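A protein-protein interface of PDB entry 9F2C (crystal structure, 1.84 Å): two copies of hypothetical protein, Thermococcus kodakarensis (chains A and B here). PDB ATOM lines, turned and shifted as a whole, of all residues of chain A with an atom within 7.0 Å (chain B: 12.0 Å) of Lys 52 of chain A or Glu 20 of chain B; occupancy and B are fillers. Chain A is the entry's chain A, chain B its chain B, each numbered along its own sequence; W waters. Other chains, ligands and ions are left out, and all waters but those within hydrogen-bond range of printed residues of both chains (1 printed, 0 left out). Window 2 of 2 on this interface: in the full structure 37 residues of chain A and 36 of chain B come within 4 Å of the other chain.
NE2 of Gln 47 of chain A lies within hydrogen-bond range of OD2 of Asp 18 of chain B (2.9 Å). The side-chain amino group (NZ) of Lys 52 of chain A lies within salt-bridge range of the side-chain carboxylate (OE1) of Glu 20 of chain B (2.8 Å). N of Arg 22 of chain B is in hydrogen-bond range of O of Lys 52 of chain A, 2.9 Å away. N of Thr 53 of chain A lies within hydrogen-bond range of SD of Met 21 of chain B, at 3.5 Å. The backbone carbonyl oxygen of Arg 22 of chain B lies within hydrogen-bond range of the backbone NH of Leu 54 of chain A (2.9 Å). The side-chain hydroxyl (OG) of Ser 24 of chain B sits at hydrogen-bond distance from the backbone carbonyl oxygen (O) of Leu 54 of chain A, 2.6 Å away. The backbone carbonyl oxygen (O) of Lys 52 of chain A sits close to the side-chain sulfur (SD) of Met 21 of chain B (3.7 Å).
No position is printed for both chains. Of the 17 pairs that touch across the chains among the printed residues, none has its exchanged pair printed and touching as well.
N of Arg 51 of chain A sits at hydrogen-bond distance from O of Ala 46 of chain A. The guanidinium group (NH1) of Arg 51 of chain A sits at hydrogen-bond distance from the side-chain hydroxyl (OH) of Tyr 55 of chain A (3.0 Å). The backbone NH of Tyr 55 of chain A is in hydrogen-bond range of a ring nitrogen (ND1) of His 58 of chain A, 3.0 Å away. OD1 of Asp 18 of chain B is in hydrogen-bond range of N of Glu 20 of chain B (3.0 Å). The backbone carbonyl oxygen (O) of Pro 19 of chain B is in hydrogen-bond range of the guanidinium group (NH1) of Arg 22 of chain B (2.9 Å). The side-chain hydroxyl of Ser 24 of chain B sits at hydrogen-bond distance from the backbone NH of Phe 27 of chain B (3.3 Å).
Met 21 of chain B touches Ala 46 of chain A. Gln 47 of chain A touches Met 21 of chain B. CE of Met 21 of chain B touches O of Arg 51 of chain A (3.4 Å). O of Arg 22 of chain B touches CA of Thr 53 of chain A (3.4 Å). Ser 24 of chain B touches Thr 53 of chain A (N to CG2, 3.96 Å). Leu 54 of chain A touches Val 14 of chain B. Met 21 of chain B touches Leu 54 of chain A (CG to CG, 3.9 Å). O of Leu 54 of chain A touches CB of Phe 27 of chain B, 3.6 Å away. Tyr 55 of chain A touches Ser 24 of chain B. Phe 27 of chain B touches Tyr 55 of chain A (CD1 to O, 3.3 Å).
Hydrophobic or aromatic side chains of chain B that line the printed part of chain A: Val 14, Met 21 and Phe 27. Of the 9 printed residues of chain A, 7 touch a printed residue of chain B.
Water W1 bridges NE2 of Gln 47 of chain A and O of Val 17 of chain B.
Of chain A, only Lys 52 comes within 4 Å of Glu 20 of chain B. Of chain B, only Met 21 comes within 4 Å of Ala 46 of chain A. Arg 51 of chain A touches one residue of chain B. Thr 53 of chain A touches three residues of chain B. Of chain B, only Val 14 (3.7 Å), Met 21 (3.9 Å), Arg 22 (2.9 Å), Ser 24 (2.6 Å) and Phe 27 (3.6 Å) come within 4 Å of Leu 54 of chain A. Of the printed residues of chain A, Phe 27 of chain B touches Leu 54 and Tyr 55. Printed residues of chain A within 4 Å of Ser 24 of chain B: Thr 53, Leu 54 and Tyr 55. Of the printed residues of chain A, Met 21 of chain B touches Ala 46 (3.8 Å), Gln 47 (3.9 Å), Arg 51 (3.4 Å), Lys 52 (3.4 Å), Thr 53 (3.5 Å) and Leu 54 (3.9 Å). Val 23 of chain B touches none of the printed residues of chain A. The nearest residue of chain B that does not touch Lys 52 of chain A is Asp 18 of chain B (4.3 Å).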
ATOM      1  N   ALA A  46      23.701 -12.503  25.244  1.00  0.00           N
ATOM      2  CA  ALA A  46      24.012 -13.952  25.216  1.00  0.00           C
ATOM      3  C   ALA A  46      25.296 -14.213  26.006  1.00  0.00           C
ATOM      4  O   ALA A  46      25.312 -15.170  26.813  1.00  0.00           O
ATOM      5  CB  ALA A  46      24.114 -14.443  23.795  1.00  0.00           C
ATOM      6  N   GLN A  47      26.317 -13.379  25.814  1.00  0.00           N
ATOM      7  CA  GLN A  47      27.616 -13.503  26.531  1.00  0.00           C
ATOM      8  C   GLN A  47      27.402 -13.328  28.040  1.00  0.00           C
ATOM      9  O   GLN A  47      28.037 -14.077  28.809  1.00  0.00           O
ATOM     10  CB  GLN A  47      28.632 -12.499  25.988  1.00  0.00           C
ATOM     11  CG  GLN A  47      29.147 -12.883  24.607  1.00  0.00           C
ATOM     12  CD  GLN A  47      30.021 -11.816  24.000  1.00  0.00           C
ATOM     13  OE1 GLN A  47      29.983 -10.653  24.395  1.00  0.00           O
ATOM     14  NE2 GLN A  47      30.814 -12.210  23.017  1.00  0.00           N
ATOM     15  N   GLY A  50      26.219 -16.419  29.479  1.00  0.00           N
ATOM     16  CA  GLY A  50      27.190 -17.519  29.301  1.00  0.00           C
ATOM     17  C   GLY A  50      26.801 -18.454  28.163  1.00  0.00           C
ATOM     18  O   GLY A  50      27.218 -19.628  28.193  1.00  0.00           O
ATOM     19  N   ARG A  51      26.028 -17.965  27.192  1.00  0.00           N
ATOM     20  CA  ARG A  51      25.553 -18.761  26.025  1.00  0.00           C
ATOM     21  C   ARG A  51      26.478 -18.514  24.829  1.00  0.00           C
ATOM     22  O   ARG A  51      27.020 -17.407  24.711  1.00  0.00           O
ATOM     23  CB  ARG A  51      24.111 -18.398  25.634  1.00  0.00           C
ATOM     24  CG  ARG A  51      23.055 -18.526  26.722  1.00  0.00           C
ATOM     25  CD  ARG A  51      23.021 -19.864  27.437  1.00  0.00           C
ATOM     26  NE  ARG A  51      22.339 -20.882  26.652  1.00  0.00           N
ATOM     27  CZ  ARG A  51      21.119 -21.363  26.889  1.00  0.00           C
ATOM     28  NH1 ARG A  51      20.623 -22.290  26.084  1.00  0.00           N
ATOM     29  NH2 ARG A  51      20.400 -20.928  27.916  1.00  0.00           N
ATOM     30  N   LYS A  52      26.610 -19.511  23.943  1.00  0.00           N
ATOM     31  CA  LYS A  52      27.347 -19.400  22.658  1.00  0.00           C
ATOM     32  C   LYS A  52      26.366 -19.550  21.494  1.00  0.00           C
ATOM     33  O   LYS A  52      26.815 -19.876  20.375  1.00  0.00           O
ATOM     34  CB  LYS A  52      28.479 -20.433  22.641  1.00  0.00           C
ATOM     35  CG  LYS A  52      29.635 -20.100  23.574  1.00  0.00           C
ATOM     36  CD  LYS A  52      30.362 -18.817  23.177  1.00  0.00           C
ATOM     37  CE  LYS A  52      31.617 -18.533  23.982  1.00  0.00           C
ATOM     38  NZ  LYS A  52      32.387 -19.755  24.290  1.00  0.00           N
ATOM     39  N   THR A  53      25.075 -19.311  21.751  1.00  0.00           N
ATOM     40  CA  THR A  53      23.985 -19.310  20.740  1.00  0.00           C
ATOM     41  C   THR A  53      23.113 -18.072  20.954  1.00  0.00           C
ATOM     42  O   THR A  53      22.726 -17.802  22.110  1.00  0.00           O
ATOM     43  CB  THR A  53      23.107 -20.563  20.825  1.00  0.00           C
ATOM     44  OG1 THR A  53      23.920 -21.726  20.676  1.00  0.00           O
ATOM     45  CG2 THR A  53      22.042 -20.602  19.749  1.00  0.00           C
ATOM     46  N   LEU A  54      22.782 -17.374  19.870  1.00  0.00           N
ATOM     47  CA  LEU A  54      21.787 -16.267  19.889  1.00  0.00           C
ATOM     48  C   LEU A  54      20.396 -16.879  19.745  1.00  0.00           C
ATOM     49  O   LEU A  54      20.155 -17.584  18.738  1.00  0.00           O
ATOM     50  CB  LEU A  54      22.068 -15.281  18.752  1.00  0.00           C
ATOM     51  CG  LEU A  54      23.359 -14.483  18.878  1.00  0.00           C
ATOM     52  CD1 LEU A  54      23.585 -13.603  17.662  1.00  0.00           C
ATOM     53  CD2 LEU A  54      23.324 -13.641  20.138  1.00  0.00           C
ATOM     54  N   TYR A  55      19.514 -16.595  20.703  1.00  0.00           N
ATOM     55  CA  TYR A  55      18.081 -16.984  20.672  1.00  0.00           C
ATOM     56  C   TYR A  55      17.241 -15.745  20.361  1.00  0.00           C
ATOM     57  O   TYR A  55      17.772 -14.618  20.499  1.00  0.00           O
ATOM     58  CB  TYR A  55      17.701 -17.620  22.004  1.00  0.00           C
ATOM     59  CG  TYR A  55      18.452 -18.898  22.284  1.00  0.00           C
ATOM     60  CD1 TYR A  55      18.309 -19.994  21.453  1.00  0.00           C
ATOM     61  CD2 TYR A  55      19.297 -19.019  23.370  1.00  0.00           C
ATOM     62  CE1 TYR A  55      18.959 -21.190  21.713  1.00  0.00           C
ATOM     63  CE2 TYR A  55      19.982 -20.197  23.630  1.00  0.00           C
ATOM     64  CZ  TYR A  55      19.800 -21.289  22.804  1.00  0.00           C
ATOM     65  OH  TYR A  55      20.470 -22.450  23.046  1.00  0.00           O
ATOM     66  N   HIS A  58      17.194 -12.865  22.808  1.00  0.00           N
ATOM     67  CA  HIS A  58      18.390 -11.990  22.934  1.00  0.00           C
ATOM     68  C   HIS A  58      18.250 -10.703  22.110  1.00  0.00           C
ATOM     69  O   HIS A  58      19.011  -9.768  22.377  1.00  0.00           O
ATOM     70  CB  HIS A  58      19.670 -12.728  22.526  1.00  0.00           C
ATOM     71  CG  HIS A  58      20.050 -13.805  23.480  1.00  0.00           C
ATOM     72  ND1 HIS A  58      20.442 -15.050  23.062  1.00  0.00           N
ATOM     73  CD2 HIS A  58      20.116 -13.817  24.826  1.00  0.00           C
ATOM     74  CE1 HIS A  58      20.732 -15.794  24.111  1.00  0.00           C
ATOM     75  NE2 HIS A  58      20.537 -15.059  25.206  1.00  0.00           N
ATOM     76  N   VAL B  10      24.292 -12.210   8.245  1.00  0.00           N
ATOM     77  CA  VAL B  10      24.067 -12.046   9.709  1.00  0.00           C
ATOM     78  C   VAL B  10      25.023 -13.001  10.428  1.00  0.00           C
ATOM     79  O   VAL B  10      25.726 -12.532  11.340  1.00  0.00           O
ATOM     80  CB  VAL B  10      22.599 -12.277  10.094  1.00  0.00           C
ATOM     81  CG1 VAL B  10      22.408 -12.288  11.603  1.00  0.00           C
ATOM     82  CG2 VAL B  10      21.678 -11.245   9.448  1.00  0.00           C
ATOM     83  N   LYS B  11      25.089 -14.264   9.987  1.00  0.00           N
ATOM     84  CA  LYS B  11      25.983 -15.294  10.593  1.00  0.00           C
ATOM     85  C   LYS B  11      27.437 -14.799  10.532  1.00  0.00           C
ATOM     86  O   LYS B  11      28.120 -14.827  11.571  1.00  0.00           O
ATOM     87  CB  LYS B  11      25.815 -16.645   9.892  1.00  0.00           C
ATOM     88  N   GLU B  12      27.876 -14.341   9.359  1.00  0.00           N
ATOM     89  CA  GLU B  12      29.248 -13.823   9.113  1.00  0.00           C
ATOM     90  C   GLU B  12      29.515 -12.638  10.050  1.00  0.00           C
ATOM     91  O   GLU B  12      30.595 -12.593  10.651  1.00  0.00           O
ATOM     92  CB  GLU B  12      29.382 -13.450   7.634  1.00  0.00           C
ATOM     93  CG  GLU B  12      30.703 -12.851   7.230  1.00  0.00           C
ATOM     94  CD  GLU B  12      30.697 -12.438   5.764  1.00  0.00           C
ATOM     95  OE1 GLU B  12      29.950 -13.066   4.967  1.00  0.00           O
ATOM     96  OE2 GLU B  12      31.410 -11.474   5.426  1.00  0.00           O
ATOM     97  N   PHE B  13      28.571 -11.708  10.190  1.00  0.00           N
ATOM     98  CA  PHE B  13      28.736 -10.520  11.070  1.00  0.00           C
ATOM     99  C   PHE B  13      28.902 -10.983  12.524  1.00  0.00           C
ATOM    100  O   PHE B  13      29.813 -10.503  13.216  1.00  0.00           O
ATOM    101  CB  PHE B  13      27.564  -9.543  10.970  1.00  0.00           C
ATOM    102  CG  PHE B  13      27.744  -8.358  11.885  1.00  0.00           C
ATOM    103  CD1 PHE B  13      28.732  -7.417  11.632  1.00  0.00           C
ATOM    104  CD2 PHE B  13      26.985  -8.227  13.040  1.00  0.00           C
ATOM    105  CE1 PHE B  13      28.928  -6.349  12.495  1.00  0.00           C
ATOM    106  CE2 PHE B  13      27.190  -7.161  13.902  1.00  0.00           C
ATOM    107  CZ  PHE B  13      28.150  -6.218  13.625  1.00  0.00           C
ATOM    108  N   VAL B  14      28.044 -11.891  12.982  1.00  0.00           N
ATOM    109  CA  VAL B  14      28.105 -12.430  14.374  1.00  0.00           C
ATOM    110  C   VAL B  14      29.505 -13.014  14.603  1.00  0.00           C
ATOM    111  O   VAL B  14      30.106 -12.722  15.656  1.00  0.00           O
ATOM    112  CB  VAL B  14      26.980 -13.447  14.620  1.00  0.00           C
ATOM    113  CG1 VAL B  14      27.195 -14.242  15.880  1.00  0.00           C
ATOM    114  CG2 VAL B  14      25.628 -12.755  14.658  1.00  0.00           C
ATOM    115  N   LYS B  15      30.023 -13.787  13.645  1.00  0.00           N
ATOM    116  CA  LYS B  15      31.357 -14.433  13.741  1.00  0.00           C
ATOM    117  C   LYS B  15      32.444 -13.356  13.853  1.00  0.00           C
ATOM    118  O   LYS B  15      33.397 -13.574  14.621  1.00  0.00           O
ATOM    119  CB  LYS B  15      31.605 -15.383  12.567  1.00  0.00           C
ATOM    120  CG  LYS B  15      30.705 -16.612  12.559  1.00  0.00           C
ATOM    121  N   SER B  16      32.300 -12.238  13.147  1.00  0.00           N
ATOM    122  CA  SER B  16      33.269 -11.107  13.164  1.00  0.00           C
ATOM    123  C   SER B  16      33.325 -10.488  14.570  1.00  0.00           C
ATOM    124  O   SER B  16      34.410 -10.011  14.945  1.00  0.00           O
ATOM    125  CB  SER B  16      32.966 -10.074  12.102  1.00  0.00           C
ATOM    126  OG  SER B  16      31.867  -9.251  12.468  1.00  0.00           O
ATOM    127  N   VAL B  17      32.217 -10.519  15.322  1.00  0.00           N
ATOM    128  CA  VAL B  17      32.136  -9.966  16.707  1.00  0.00           C
ATOM    129  C   VAL B  17      32.601 -11.033  17.706  1.00  0.00           C
ATOM    130  O   VAL B  17      33.444 -10.714  18.556  1.00  0.00           O
ATOM    131  CB  VAL B  17      30.719  -9.449  17.030  1.00  0.00           C
ATOM    132  CG1 VAL B  17      30.634  -8.915  18.453  1.00  0.00           C
ATOM    133  CG2 VAL B  17      30.253  -8.393  16.034  1.00  0.00           C
ATOM    134  N   ASP B  18      32.061 -12.249  17.631  1.00  0.00           N
ATOM    135  CA  ASP B  18      32.408 -13.360  18.559  1.00  0.00           C
ATOM    136  C   ASP B  18      32.544 -14.633  17.741  1.00  0.00           C
ATOM    137  O   ASP B  18      31.545 -15.206  17.347  1.00  0.00           O
ATOM    138  CB  ASP B  18      31.383 -13.511  19.687  1.00  0.00           C
ATOM    139  CG  ASP B  18      31.624 -14.696  20.624  1.00  0.00           C
ATOM    140  OD1 ASP B  18      32.535 -15.517  20.350  1.00  0.00           O
ATOM    141  OD2 ASP B  18      30.889 -14.808  21.622  1.00  0.00           O
ATOM    142  N   PRO B  19      33.786 -15.099  17.464  1.00  0.00           N
ATOM    143  CA  PRO B  19      34.033 -16.306  16.671  1.00  0.00           C
ATOM    144  C   PRO B  19      33.310 -17.581  17.110  1.00  0.00           C
ATOM    145  O   PRO B  19      33.141 -18.436  16.274  1.00  0.00           O
ATOM    146  CB  PRO B  19      35.542 -16.552  16.830  1.00  0.00           C
ATOM    147  CG  PRO B  19      36.112 -15.178  17.096  1.00  0.00           C
ATOM    148  CD  PRO B  19      35.033 -14.439  17.865  1.00  0.00           C
ATOM    149  N   GLU B  20      32.948 -17.706  18.395  1.00  0.00           N
ATOM    150  CA  GLU B  20      32.318 -18.937  18.950  1.00  0.00           C
ATOM    151  C   GLU B  20      30.791 -18.825  18.953  1.00  0.00           C
ATOM    152  O   GLU B  20      30.140 -19.835  19.243  1.00  0.00           O
ATOM    153  CB  GLU B  20      32.819 -19.193  20.371  1.00  0.00           C
ATOM    154  CG  GLU B  20      34.326 -19.363  20.437  1.00  0.00           C
ATOM    155  CD  GLU B  20      34.888 -19.456  21.840  1.00  0.00           C
ATOM    156  OE1 GLU B  20      34.505 -20.395  22.566  1.00  0.00           O
ATOM    157  OE2 GLU B  20      35.717 -18.587  22.198  1.00  0.00           O
ATOM    158  N   MET B  21      30.239 -17.644  18.664  1.00  0.00           N
ATOM    159  CA  MET B  21      28.781 -17.386  18.789  1.00  0.00           C
ATOM    160  C   MET B  21      28.072 -17.917  17.535  1.00  0.00           C
ATOM    161  O   MET B  21      28.464 -17.564  16.413  1.00  0.00           O
ATOM    162  CB  MET B  21      28.498 -15.892  18.966  1.00  0.00           C
ATOM    163  CG  MET B  21      27.046 -15.552  19.289  1.00  0.00           C
ATOM    164  SD  MET B  21      26.469 -16.249  20.843  1.00  0.00           S
ATOM    165  CE  MET B  21      27.368 -15.268  22.040  1.00  0.00           C
ATOM    166  N   ARG B  22      27.086 -18.789  17.733  1.00  0.00           N
ATOM    167  CA  ARG B  22      26.235 -19.343  16.655  1.00  0.00           C
ATOM    168  C   ARG B  22      24.890 -18.619  16.706  1.00  0.00           C
ATOM    169  O   ARG B  22      24.637 -17.883  17.675  1.00  0.00           O
ATOM    170  CB  ARG B  22      26.133 -20.867  16.799  1.00  0.00           C
ATOM    171  CG  ARG B  22      27.462 -21.586  16.600  1.00  0.00           C
ATOM    172  CD  ARG B  22      28.256 -21.180  15.357  1.00  0.00           C
ATOM    173  NE  ARG B  22      29.659 -21.597  15.420  1.00  0.00           N
ATOM    174  CZ  ARG B  22      30.716 -20.780  15.507  1.00  0.00           C
ATOM    175  NH1 ARG B  22      30.570 -19.460  15.518  1.00  0.00           N
ATOM    176  NH2 ARG B  22      31.935 -21.292  15.555  1.00  0.00           N
ATOM    177  N   VAL B  23      24.079 -18.777  15.667  1.00  0.00           N
ATOM    178  CA  VAL B  23      22.764 -18.102  15.522  1.00  0.00           C
ATOM    179  C   VAL B  23      21.687 -19.178  15.371  1.00  0.00           C
ATOM    180  O   VAL B  23      21.763 -19.951  14.399  1.00  0.00           O
ATOM    181  CB  VAL B  23      22.772 -17.143  14.318  1.00  0.00           C
ATOM    182  CG1 VAL B  23      21.480 -16.352  14.212  1.00  0.00           C
ATOM    183  CG2 VAL B  23      23.971 -16.213  14.335  1.00  0.00           C
ATOM    184  N   SER B  24      20.716 -19.216  16.287  1.00  0.00           N
ATOM    185  CA  SER B  24      19.532 -20.106  16.188  1.00  0.00           C
ATOM    186  C   SER B  24      18.692 -19.657  14.998  1.00  0.00           C
ATOM    187  O   SER B  24      18.644 -18.466  14.680  1.00  0.00           O
ATOM    188  CB  SER B  24      18.734 -20.117  17.459  1.00  0.00           C
ATOM    189  OG  SER B  24      18.103 -18.865  17.657  1.00  0.00           O
ATOM    190  N   PRO B  25      17.997 -20.576  14.300  1.00  0.00           N
ATOM    191  CA  PRO B  25      17.094 -20.180  13.218  1.00  0.00           C
ATOM    192  C   PRO B  25      16.068 -19.116  13.651  1.00  0.00           C
ATOM    193  O   PRO B  25      15.762 -18.239  12.860  1.00  0.00           O
ATOM    194  CB  PRO B  25      16.416 -21.503  12.829  1.00  0.00           C
ATOM    195  CG  PRO B  25      17.430 -22.566  13.209  1.00  0.00           C
ATOM    196  CD  PRO B  25      18.075 -22.036  14.472  1.00  0.00           C
ATOM    197  N   PHE B  27      16.330 -16.733  15.811  1.00  0.00           N
ATOM    198  CA  PHE B  27      16.969 -15.403  15.979  1.00  0.00           C
ATOM    199  C   PHE B  27      16.809 -14.592  14.696  1.00  0.00           C
ATOM    200  O   PHE B  27      16.456 -13.401  14.773  1.00  0.00           O
ATOM    201  CB  PHE B  27      18.448 -15.506  16.360  1.00  0.00           C
ATOM    202  CG  PHE B  27      19.097 -14.153  16.479  1.00  0.00           C
ATOM    203  CD1 PHE B  27      18.967 -13.417  17.650  1.00  0.00           C
ATOM    204  CD2 PHE B  27      19.749 -13.569  15.404  1.00  0.00           C
ATOM    205  CE1 PHE B  27      19.538 -12.157  17.767  1.00  0.00           C
ATOM    206  CE2 PHE B  27      20.314 -12.308  15.524  1.00  0.00           C
ATOM    207  CZ  PHE B  27      20.208 -11.606  16.700  1.00  0.00           C
ATOM    208  N   TYR B  28      17.058 -15.207  13.538  1.00  0.00           N
ATOM    209  CA  TYR B  28      16.935 -14.527  12.219  1.00  0.00           C
ATOM    210  C   TYR B  28      15.519 -13.968  12.061  1.00  0.00           C
ATOM    211  O   TYR B  28      15.391 -12.818  11.625  1.00  0.00           O
ATOM    212  CB  TYR B  28      17.261 -15.453  11.044  1.00  0.00           C
ATOM    213  CG  TYR B  28      18.664 -15.995  11.041  1.00  0.00           C
ATOM    214  CD1 TYR B  28      19.749 -15.188  10.751  1.00  0.00           C
ATOM    215  CD2 TYR B  28      18.891 -17.348  11.203  1.00  0.00           C
ATOM    216  CE1 TYR B  28      21.034 -15.706  10.726  1.00  0.00           C
ATOM    217  CE2 TYR B  28      20.171 -17.883  11.146  1.00  0.00           C
ATOM    218  CZ  TYR B  28      21.244 -17.064  10.858  1.00  0.00           C
ATOM    219  OH  TYR B  28      22.529 -17.528  10.807  1.00  0.00           O
HETATM  220  O   HOH W   1      32.605 -10.743  21.384  1.00  0.00           O
